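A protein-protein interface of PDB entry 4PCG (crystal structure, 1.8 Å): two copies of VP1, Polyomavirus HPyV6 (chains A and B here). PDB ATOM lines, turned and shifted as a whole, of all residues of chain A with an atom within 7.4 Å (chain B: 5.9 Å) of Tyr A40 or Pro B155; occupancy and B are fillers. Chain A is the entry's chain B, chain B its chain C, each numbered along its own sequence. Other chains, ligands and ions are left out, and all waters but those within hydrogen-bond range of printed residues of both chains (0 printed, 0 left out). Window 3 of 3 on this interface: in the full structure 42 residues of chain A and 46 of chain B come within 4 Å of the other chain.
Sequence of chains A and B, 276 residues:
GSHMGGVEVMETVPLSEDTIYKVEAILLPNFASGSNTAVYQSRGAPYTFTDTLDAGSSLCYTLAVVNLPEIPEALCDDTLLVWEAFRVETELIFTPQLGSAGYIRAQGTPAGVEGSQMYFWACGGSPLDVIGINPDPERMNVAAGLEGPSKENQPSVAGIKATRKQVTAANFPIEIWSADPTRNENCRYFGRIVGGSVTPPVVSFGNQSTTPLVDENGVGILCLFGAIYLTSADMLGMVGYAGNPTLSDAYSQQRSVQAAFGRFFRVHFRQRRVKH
The side-chain hydroxyl (OG) of Ser A42 lies within hydrogen-bond range of the backbone carbonyl oxygen (O) of Ser B156 (2.7 Å).
The side-chain hydroxyl (OG1) of Thr A62 sits at hydrogen-bond distance from the backbone carbonyl oxygen (O) of Leu A28 (2.6 Å). O of Pro A29 sits at hydrogen-bond distance from N of Gln A41, at 3.2 Å. NE2 of Gln A41 lies within hydrogen-bond range of O of Arg A43, 2.8 Å away.
Ile A26 touches Ala B158. Leu A28 touches Val B157. Leu A28 touches Ala B158. Pro A29 touches Val B157. Tyr A40 touches Pro B155. C of Tyr A40 touches CG1 of Val B157 (3.9 Å). Ser B156 touches Gln A41 (OG to CA, 3.9 Å). Gln A41 touches Val B157 (CA to CG1, 3.7 Å). Ser A42 touches Val B157.
Of the printed residues of chain B, Ile A26 touches Ala B158. Printed residues of chain B within 4 Å of Leu A28: Val B157 and Ala B158. Of the printed residues of chain B, Tyr A40 touches Pro B155 (3.5 Å) and Val B157 (3.9 Å). Of the printed residues of chain B, Gln A41 touches Ser B156 (3.9 Å) and Val B157 (3.7 Å). Of the printed residues of chain B, Ser A42 touches Ser B156 and Val B157. Pro B155 touches just one residue of chain A: Tyr A40 (3.5 Å). Printed residues of chain A within 4 Å of Val B157: Leu A28 (3.9 Å), Pro A29 (3.6 Å), Tyr A40 (3.9 Å), Gln A41 (3.7 Å) and Ser A42 (3.8 Å). The nearest residue of chain B that does not touch Tyr A40 is Ser B156 (5.0 Å). The nearest printed residue of chain B that does not touch Pro A29 is Ser B156 (5.4 Å).
Hydrophobic or aromatic side chains of chain B within 4 Å of the printed part of chain A: Pro B155 and Val B157. Of the 18 printed residues of chain A, 6 touch a printed residue of chain B. Hydrophobic or aromatic side chains of chain A within 4 Å of the printed part of chain B: Ile A26, Leu A28 and Pro A29. Among the printed residues, 10 pairs touch across the chains.
No position is printed for both chains.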
ATOM      1  N   ILE A  26      18.280 -31.769   5.287  1.00  0.00           N
ATOM      2  CA  ILE A  26      18.773 -30.498   4.761  1.00  0.00           C
ATOM      3  C   ILE A  26      20.279 -30.550   4.867  1.00  0.00           C
ATOM      4  O   ILE A  26      20.810 -30.661   5.971  1.00  0.00           O
ATOM      5  CB  ILE A  26      18.223 -29.277   5.510  1.00  0.00           C
ATOM      6  CG1 ILE A  26      16.716 -29.152   5.264  1.00  0.00           C
ATOM      7  CG2 ILE A  26      18.918 -27.999   5.022  1.00  0.00           C
ATOM      8  CD1 ILE A  26      16.044 -28.063   6.047  1.00  0.00           C
ATOM      9  N   LEU A  27      20.942 -30.533   3.713  1.00  0.00           N
ATOM     10  CA  LEU A  27      22.383 -30.558   3.640  1.00  0.00           C
ATOM     11  C   LEU A  27      22.822 -29.112   3.818  1.00  0.00           C
ATOM     12  O   LEU A  27      22.279 -28.237   3.154  1.00  0.00           O
ATOM     13  CB  LEU A  27      22.840 -31.149   2.290  1.00  0.00           C
ATOM     14  CG  LEU A  27      23.051 -32.663   2.368  1.00  0.00           C
ATOM     15  CD1 LEU A  27      21.786 -33.412   2.728  1.00  0.00           C
ATOM     16  CD2 LEU A  27      23.699 -33.172   1.094  1.00  0.00           C
ATOM     17  N   LEU A  28      23.769 -28.878   4.723  1.00  0.00           N
ATOM     18  CA  LEU A  28      24.172 -27.532   5.120  1.00  0.00           C
ATOM     19  C   LEU A  28      25.506 -27.174   4.466  1.00  0.00           C
ATOM     20  O   LEU A  28      26.360 -28.045   4.266  1.00  0.00           O
ATOM     21  CB  LEU A  28      24.279 -27.454   6.638  1.00  0.00           C
ATOM     22  CG  LEU A  28      23.031 -27.904   7.415  1.00  0.00           C
ATOM     23  CD1 LEU A  28      23.364 -27.991   8.875  1.00  0.00           C
ATOM     24  CD2 LEU A  28      21.871 -26.956   7.143  1.00  0.00           C
ATOM     25  N   PRO A  29      25.693 -25.880   4.112  1.00  0.00           N
ATOM     26  CA  PRO A  29      26.930 -25.488   3.447  1.00  0.00           C
ATOM     27  C   PRO A  29      28.161 -25.729   4.332  1.00  0.00           C
ATOM     28  O   PRO A  29      28.123 -25.534   5.529  1.00  0.00           O
ATOM     29  CB  PRO A  29      26.729 -24.001   3.169  1.00  0.00           C
ATOM     30  CG  PRO A  29      25.751 -23.543   4.186  1.00  0.00           C
ATOM     31  CD  PRO A  29      24.826 -24.726   4.390  1.00  0.00           C
ATOM     32  N   ASN A  30      29.262 -26.089   3.696  1.00  0.00           N
ATOM     33  CA  ASN A  30      30.422 -26.587   4.392  1.00  0.00           C
ATOM     34  C   ASN A  30      31.707 -26.001   3.802  1.00  0.00           C
ATOM     35  O   ASN A  30      32.041 -26.273   2.652  1.00  0.00           O
ATOM     36  CB  ASN A  30      30.388 -28.101   4.189  1.00  0.00           C
ATOM     37  CG  ASN A  30      31.668 -28.763   4.526  1.00  0.00           C
ATOM     38  OD1 ASN A  30      32.372 -28.371   5.488  1.00  0.00           O
ATOM     39  ND2 ASN A  30      32.012 -29.786   3.743  1.00  0.00           N
ATOM     40  N   PHE A  31      32.395 -25.202   4.599  1.00  0.00           N
ATOM     41  CA  PHE A  31      33.722 -24.627   4.302  1.00  0.00           C
ATOM     42  C   PHE A  31      34.725 -25.278   5.265  1.00  0.00           C
ATOM     43  O   PHE A  31      35.309 -24.630   6.159  1.00  0.00           O
ATOM     44  CB  PHE A  31      33.700 -23.096   4.533  1.00  0.00           C
ATOM     45  CG  PHE A  31      32.862 -22.323   3.533  1.00  0.00           C
ATOM     46  CD1 PHE A  31      31.508 -22.071   3.779  1.00  0.00           C
ATOM     47  CD2 PHE A  31      33.419 -21.834   2.360  1.00  0.00           C
ATOM     48  CE1 PHE A  31      30.732 -21.363   2.879  1.00  0.00           C
ATOM     49  CE2 PHE A  31      32.650 -21.119   1.450  1.00  0.00           C
ATOM     50  CZ  PHE A  31      31.316 -20.866   1.713  1.00  0.00           C
ATOM     51  N   ALA A  32      34.870 -26.589   5.141  1.00  0.00           N
ATOM     52  CA  ALA A  32      35.714 -27.371   6.057  1.00  0.00           C
ATOM     53  C   ALA A  32      37.150 -26.898   6.142  1.00  0.00           C
ATOM     54  O   ALA A  32      37.685 -26.381   5.183  1.00  0.00           O
ATOM     55  CB  ALA A  32      35.686 -28.830   5.638  1.00  0.00           C
ATOM     56  N   THR A  37      35.845 -32.756   9.942  1.00  0.00           N
ATOM     57  CA  THR A  37      35.295 -31.584  10.615  1.00  0.00           C
ATOM     58  C   THR A  37      34.685 -30.609   9.599  1.00  0.00           C
ATOM     59  O   THR A  37      35.298 -29.583   9.196  1.00  0.00           O
ATOM     60  CB  THR A  37      36.353 -30.889  11.518  1.00  0.00           C
ATOM     61  OG1 THR A  37      37.600 -30.722  10.813  1.00  0.00           O
ATOM     62  CG2 THR A  37      36.593 -31.728  12.766  1.00  0.00           C
ATOM     63  N   ALA A  38      33.463 -30.950   9.187  1.00  0.00           N
ATOM     64  CA  ALA A  38      32.658 -30.032   8.376  1.00  0.00           C
ATOM     65  C   ALA A  38      32.409 -28.757   9.192  1.00  0.00           C
ATOM     66  O   ALA A  38      32.289 -28.789  10.441  1.00  0.00           O
ATOM     67  CB  ALA A  38      31.345 -30.665   7.939  1.00  0.00           C
ATOM     68  N   VAL A  39      32.369 -27.621   8.504  1.00  0.00           N
ATOM     69  CA  VAL A  39      32.156 -26.363   9.214  1.00  0.00           C
ATOM     70  C   VAL A  39      30.926 -25.745   8.611  1.00  0.00           C
ATOM     71  O   VAL A  39      30.981 -25.233   7.448  1.00  0.00           O
ATOM     72  CB  VAL A  39      33.390 -25.440   9.115  1.00  0.00           C
ATOM     73  CG1 VAL A  39      33.067 -24.036   9.638  1.00  0.00           C
ATOM     74  CG2 VAL A  39      34.564 -26.046   9.882  1.00  0.00           C
ATOM     75  N   TYR A  40      29.807 -25.773   9.353  1.00  0.00           N
ATOM     76  CA  TYR A  40      28.581 -25.342   8.680  1.00  0.00           C
ATOM     77  C   TYR A  40      28.390 -23.858   8.829  1.00  0.00           C
ATOM     78  O   TYR A  40      28.190 -23.345   9.929  1.00  0.00           O
ATOM     79  CB  TYR A  40      27.357 -26.121   9.126  1.00  0.00           C
ATOM     80  CG  TYR A  40      27.488 -27.600   8.930  1.00  0.00           C
ATOM     81  CD1 TYR A  40      27.734 -28.146   7.677  1.00  0.00           C
ATOM     82  CD2 TYR A  40      27.328 -28.464  10.007  1.00  0.00           C
ATOM     83  CE1 TYR A  40      27.823 -29.507   7.493  1.00  0.00           C
ATOM     84  CE2 TYR A  40      27.434 -29.824   9.843  1.00  0.00           C
ATOM     85  CZ  TYR A  40      27.680 -30.339   8.599  1.00  0.00           C
ATOM     86  OH  TYR A  40      27.784 -31.695   8.456  1.00  0.00           O
ATOM     87  N   GLN A  41      28.526 -23.168   7.713  1.00  0.00           N
ATOM     88  CA  GLN A  41      28.343 -21.731   7.669  1.00  0.00           C
ATOM     89  C   GLN A  41      28.019 -21.361   6.239  1.00  0.00           C
ATOM     90  O   GLN A  41      28.482 -22.002   5.301  1.00  0.00           O
ATOM     91  CB  GLN A  41      29.580 -20.998   8.173  1.00  0.00           C
ATOM     92  CG  GLN A  41      30.877 -21.246   7.417  1.00  0.00           C
ATOM     93  CD  GLN A  41      32.044 -20.635   8.204  1.00  0.00           C
ATOM     94  OE1 GLN A  41      32.244 -20.975   9.380  1.00  0.00           O
ATOM     95  NE2 GLN A  41      32.763 -19.681   7.599  1.00  0.00           N
ATOM     96  N   SER A  42      27.189 -20.343   6.070  1.00  0.00           N
ATOM     97  CA  SER A  42      26.743 -19.991   4.716  1.00  0.00           C
ATOM     98  C   SER A  42      27.636 -18.975   4.009  1.00  0.00           C
ATOM     99  O   SER A  42      27.489 -18.791   2.805  1.00  0.00           O
ATOM    100  CB  SER A  42      25.287 -19.507   4.737  1.00  0.00           C
ATOM    101  OG  SER A  42      25.085 -18.470   5.668  1.00  0.00           O
ATOM    102  N   ARG A  43      28.549 -18.329   4.747  1.00  0.00           N
ATOM    103  CA  ARG A  43      29.596 -17.484   4.134  1.00  0.00           C
ATOM    104  C   ARG A  43      30.943 -17.992   4.571  1.00  0.00           C
ATOM    105  O   ARG A  43      31.136 -18.297   5.743  1.00  0.00           O
ATOM    106  CB  ARG A  43      29.431 -16.022   4.549  1.00  0.00           C
ATOM    107  CG  ARG A  43      28.203 -15.405   3.908  1.00  0.00           C
ATOM    108  CD  ARG A  43      28.001 -13.973   4.352  1.00  0.00           C
ATOM    109  NE  ARG A  43      26.828 -13.391   3.704  1.00  0.00           N
ATOM    110  CZ  ARG A  43      26.506 -12.117   3.754  1.00  0.00           C
ATOM    111  NH1 ARG A  43      27.235 -11.258   4.445  1.00  0.00           N
ATOM    112  NH2 ARG A  43      25.444 -11.696   3.111  1.00  0.00           N
ATOM    113  N   TYR A  61      31.989 -29.802  -1.125  1.00  0.00           N
ATOM    114  CA  TYR A  61      30.739 -30.571  -1.178  1.00  0.00           C
ATOM    115  C   TYR A  61      30.278 -30.890   0.242  1.00  0.00           C
ATOM    116  O   TYR A  61      31.097 -31.123   1.163  1.00  0.00           O
ATOM    117  CB  TYR A  61      30.935 -31.878  -1.935  1.00  0.00           C
ATOM    118  CG  TYR A  61      31.098 -31.770  -3.423  1.00  0.00           C
ATOM    119  CD1 TYR A  61      29.984 -31.644  -4.254  1.00  0.00           C
ATOM    120  CD2 TYR A  61      32.335 -31.837  -4.008  1.00  0.00           C
ATOM    121  CE1 TYR A  61      30.116 -31.582  -5.614  1.00  0.00           C
ATOM    122  CE2 TYR A  61      32.486 -31.781  -5.379  1.00  0.00           C
ATOM    123  CZ  TYR A  61      31.362 -31.635  -6.183  1.00  0.00           C
ATOM    124  OH  TYR A  61      31.538 -31.589  -7.542  1.00  0.00           O
ATOM    125  N   THR A  62      28.967 -30.907   0.413  1.00  0.00           N
ATOM    126  CA  THR A  62      28.362 -31.455   1.618  1.00  0.00           C
ATOM    127  C   THR A  62      27.854 -32.845   1.332  1.00  0.00           C
ATOM    128  O   THR A  62      27.306 -33.077   0.276  1.00  0.00           O
ATOM    129  CB  THR A  62      27.191 -30.598   2.086  1.00  0.00           C
ATOM    130  OG1 THR A  62      27.660 -29.268   2.321  1.00  0.00           O
ATOM    131  CG2 THR A  62      26.550 -31.182   3.388  1.00  0.00           C
ATOM    132  N   LEU A  63      28.085 -33.765   2.264  1.00  0.00           N
ATOM    133  CA  LEU A  63      27.618 -35.145   2.106  1.00  0.00           C
ATOM    134  C   LEU A  63      26.748 -35.577   3.298  1.00  0.00           C
ATOM    135  O   LEU A  63      26.991 -35.195   4.455  1.00  0.00           O
ATOM    136  CB  LEU A  63      28.792 -36.090   1.898  1.00  0.00           C
ATOM    137  CG  LEU A  63      29.708 -36.534   3.023  1.00  0.00           C
ATOM    138  CD1 LEU A  63      29.164 -37.757   3.760  1.00  0.00           C
ATOM    139  CD2 LEU A  63      31.069 -36.898   2.454  1.00  0.00           C
ATOM    140  N   ALA A 170      34.509 -34.254   4.246  1.00  0.00           N
ATOM    141  CA  ALA A 170      34.029 -32.877   4.246  1.00  0.00           C
ATOM    142  C   ALA A 170      34.956 -31.925   3.491  1.00  0.00           C
ATOM    143  O   ALA A 170      34.631 -30.750   3.346  1.00  0.00           O
ATOM    144  CB  ALA A 170      33.885 -32.381   5.693  1.00  0.00           C
ATOM    145  N   ILE B 133      17.045 -16.737   9.384  1.00  0.00           N
ATOM    146  CA  ILE B 133      18.507 -16.818   9.440  1.00  0.00           C
ATOM    147  C   ILE B 133      19.162 -15.455   9.250  1.00  0.00           C
ATOM    148  O   ILE B 133      18.817 -14.710   8.343  1.00  0.00           O
ATOM    149  CB  ILE B 133      19.031 -17.804   8.372  1.00  0.00           C
ATOM    150  CG1 ILE B 133      18.488 -19.211   8.675  1.00  0.00           C
ATOM    151  CG2 ILE B 133      20.566 -17.834   8.335  1.00  0.00           C
ATOM    152  CD1 ILE B 133      18.771 -20.219   7.591  1.00  0.00           C
ATOM    153  N   PRO B 137      25.899 -12.883  11.239  1.00  0.00           N
ATOM    154  CA  PRO B 137      25.544 -12.583  12.622  1.00  0.00           C
ATOM    155  C   PRO B 137      26.652 -11.892  13.438  1.00  0.00           C
ATOM    156  O   PRO B 137      26.347 -11.257  14.428  1.00  0.00           O
ATOM    157  CB  PRO B 137      25.172 -13.962  13.196  1.00  0.00           C
ATOM    158  CG  PRO B 137      25.904 -14.938  12.357  1.00  0.00           C
ATOM    159  CD  PRO B 137      25.989 -14.332  10.985  1.00  0.00           C
ATOM    160  N   ASN B 153      23.287 -18.469  19.420  1.00  0.00           N
ATOM    161  CA  ASN B 153      24.609 -18.855  18.916  1.00  0.00           C
ATOM    162  C   ASN B 153      24.564 -19.881  17.785  1.00  0.00           C
ATOM    163  O   ASN B 153      25.581 -20.520  17.476  1.00  0.00           O
ATOM    164  CB  ASN B 153      25.496 -19.370  20.043  1.00  0.00           C
ATOM    165  CG  ASN B 153      25.907 -18.272  20.994  1.00  0.00           C
ATOM    166  OD1 ASN B 153      26.086 -17.123  20.590  1.00  0.00           O
ATOM    167  ND2 ASN B 153      26.070 -18.617  22.257  1.00  0.00           N
ATOM    168  N   GLN B 154      23.404 -20.023  17.162  1.00  0.00           N
ATOM    169  CA  GLN B 154      23.271 -20.993  16.065  1.00  0.00           C
ATOM    170  C   GLN B 154      24.049 -20.529  14.846  1.00  0.00           C
ATOM    171  O   GLN B 154      24.159 -19.315  14.578  1.00  0.00           O
ATOM    172  CB  GLN B 154      21.811 -21.249  15.691  1.00  0.00           C
ATOM    173  CG  GLN B 154      21.049 -20.094  15.065  1.00  0.00           C
ATOM    174  CD  GLN B 154      20.422 -19.160  16.091  1.00  0.00           C
ATOM    175  OE1 GLN B 154      20.963 -18.977  17.188  1.00  0.00           O
ATOM    176  NE2 GLN B 154      19.294 -18.548  15.732  1.00  0.00           N
ATOM    177  N   PRO B 155      24.588 -21.490  14.082  1.00  0.00           N
ATOM    178  CA  PRO B 155      25.214 -21.090  12.820  1.00  0.00           C
ATOM    179  C   PRO B 155      24.204 -20.531  11.802  1.00  0.00           C
ATOM    180  O   PRO B 155      23.010 -20.775  11.923  1.00  0.00           O
ATOM    181  CB  PRO B 155      25.886 -22.398  12.329  1.00  0.00           C
ATOM    182  CG  PRO B 155      25.166 -23.491  13.038  1.00  0.00           C
ATOM    183  CD  PRO B 155      24.784 -22.920  14.377  1.00  0.00           C
ATOM    184  N   SER B 156      24.715 -19.805  10.802  1.00  0.00           N
ATOM    185  CA  SER B 156      23.931 -19.125   9.779  1.00  0.00           C
ATOM    186  C   SER B 156      23.441 -20.068   8.650  1.00  0.00           C
ATOM    187  O   SER B 156      23.595 -19.774   7.447  1.00  0.00           O
ATOM    188  CB  SER B 156      24.824 -18.088   9.138  1.00  0.00           C
ATOM    189  OG  SER B 156      26.055 -18.725   8.769  1.00  0.00           O
ATOM    190  N   VAL B 157      22.859 -21.192   9.047  1.00  0.00           N
ATOM    191  CA  VAL B 157      22.421 -22.200   8.091  1.00  0.00           C
ATOM    192  C   VAL B 157      21.043 -22.729   8.501  1.00  0.00           C
ATOM    193  O   VAL B 157      20.586 -22.508   9.617  1.00  0.00           O
ATOM    194  CB  VAL B 157      23.421 -23.369   7.996  1.00  0.00           C
ATOM    195  CG1 VAL B 157      24.788 -22.898   7.567  1.00  0.00           C
ATOM    196  CG2 VAL B 157      23.543 -24.137   9.312  1.00  0.00           C
ATOM    197  N   ALA B 158      20.393 -23.444   7.595  1.00  0.00           N
ATOM    198  CA  ALA B 158      19.052 -23.935   7.844  1.00  0.00           C
ATOM    199  C   ALA B 158      19.028 -25.287   8.532  1.00  0.00           C
ATOM    200  O   ALA B 158      18.392 -26.225   8.069  1.00  0.00           O
ATOM    201  CB  ALA B 158      18.254 -23.947   6.540  1.00  0.00           C
ATOM    202  N   LYS B 161      18.830 -26.148  14.580  1.00  0.00           N
ATOM    203  CA  LYS B 161      18.841 -25.053  15.541  1.00  0.00           C
ATOM    204  C   LYS B 161      18.325 -23.727  14.968  1.00  0.00           C
ATOM    205  O   LYS B 161      18.239 -22.742  15.706  1.00  0.00           O
ATOM    206  CB  LYS B 161      20.257 -24.832  16.078  1.00  0.00           C
ATOM    207  CG  LYS B 161      20.870 -26.014  16.816  1.00  0.00           C
ATOM    208  CD  LYS B 161      22.359 -25.754  17.039  1.00  0.00           C
ATOM    209  CE  LYS B 161      23.174 -27.035  17.077  1.00  0.00           C
ATOM    210  NZ  LYS B 161      24.616 -26.722  16.858  1.00  0.00           N
ATOM    211  N   ALA B 162      17.975 -23.673  13.679  1.00  0.00           N
ATOM    212  CA  ALA B 162      17.548 -22.413  13.089  1.00  0.00           C
ATOM    213  C   ALA B 162      16.166 -22.012  13.629  1.00  0.00           C
ATOM    214  O   ALA B 162      15.345 -22.865  13.990  1.00  0.00           O
ATOM    215  CB  ALA B 162      17.549 -22.465  11.582  1.00  0.00           C
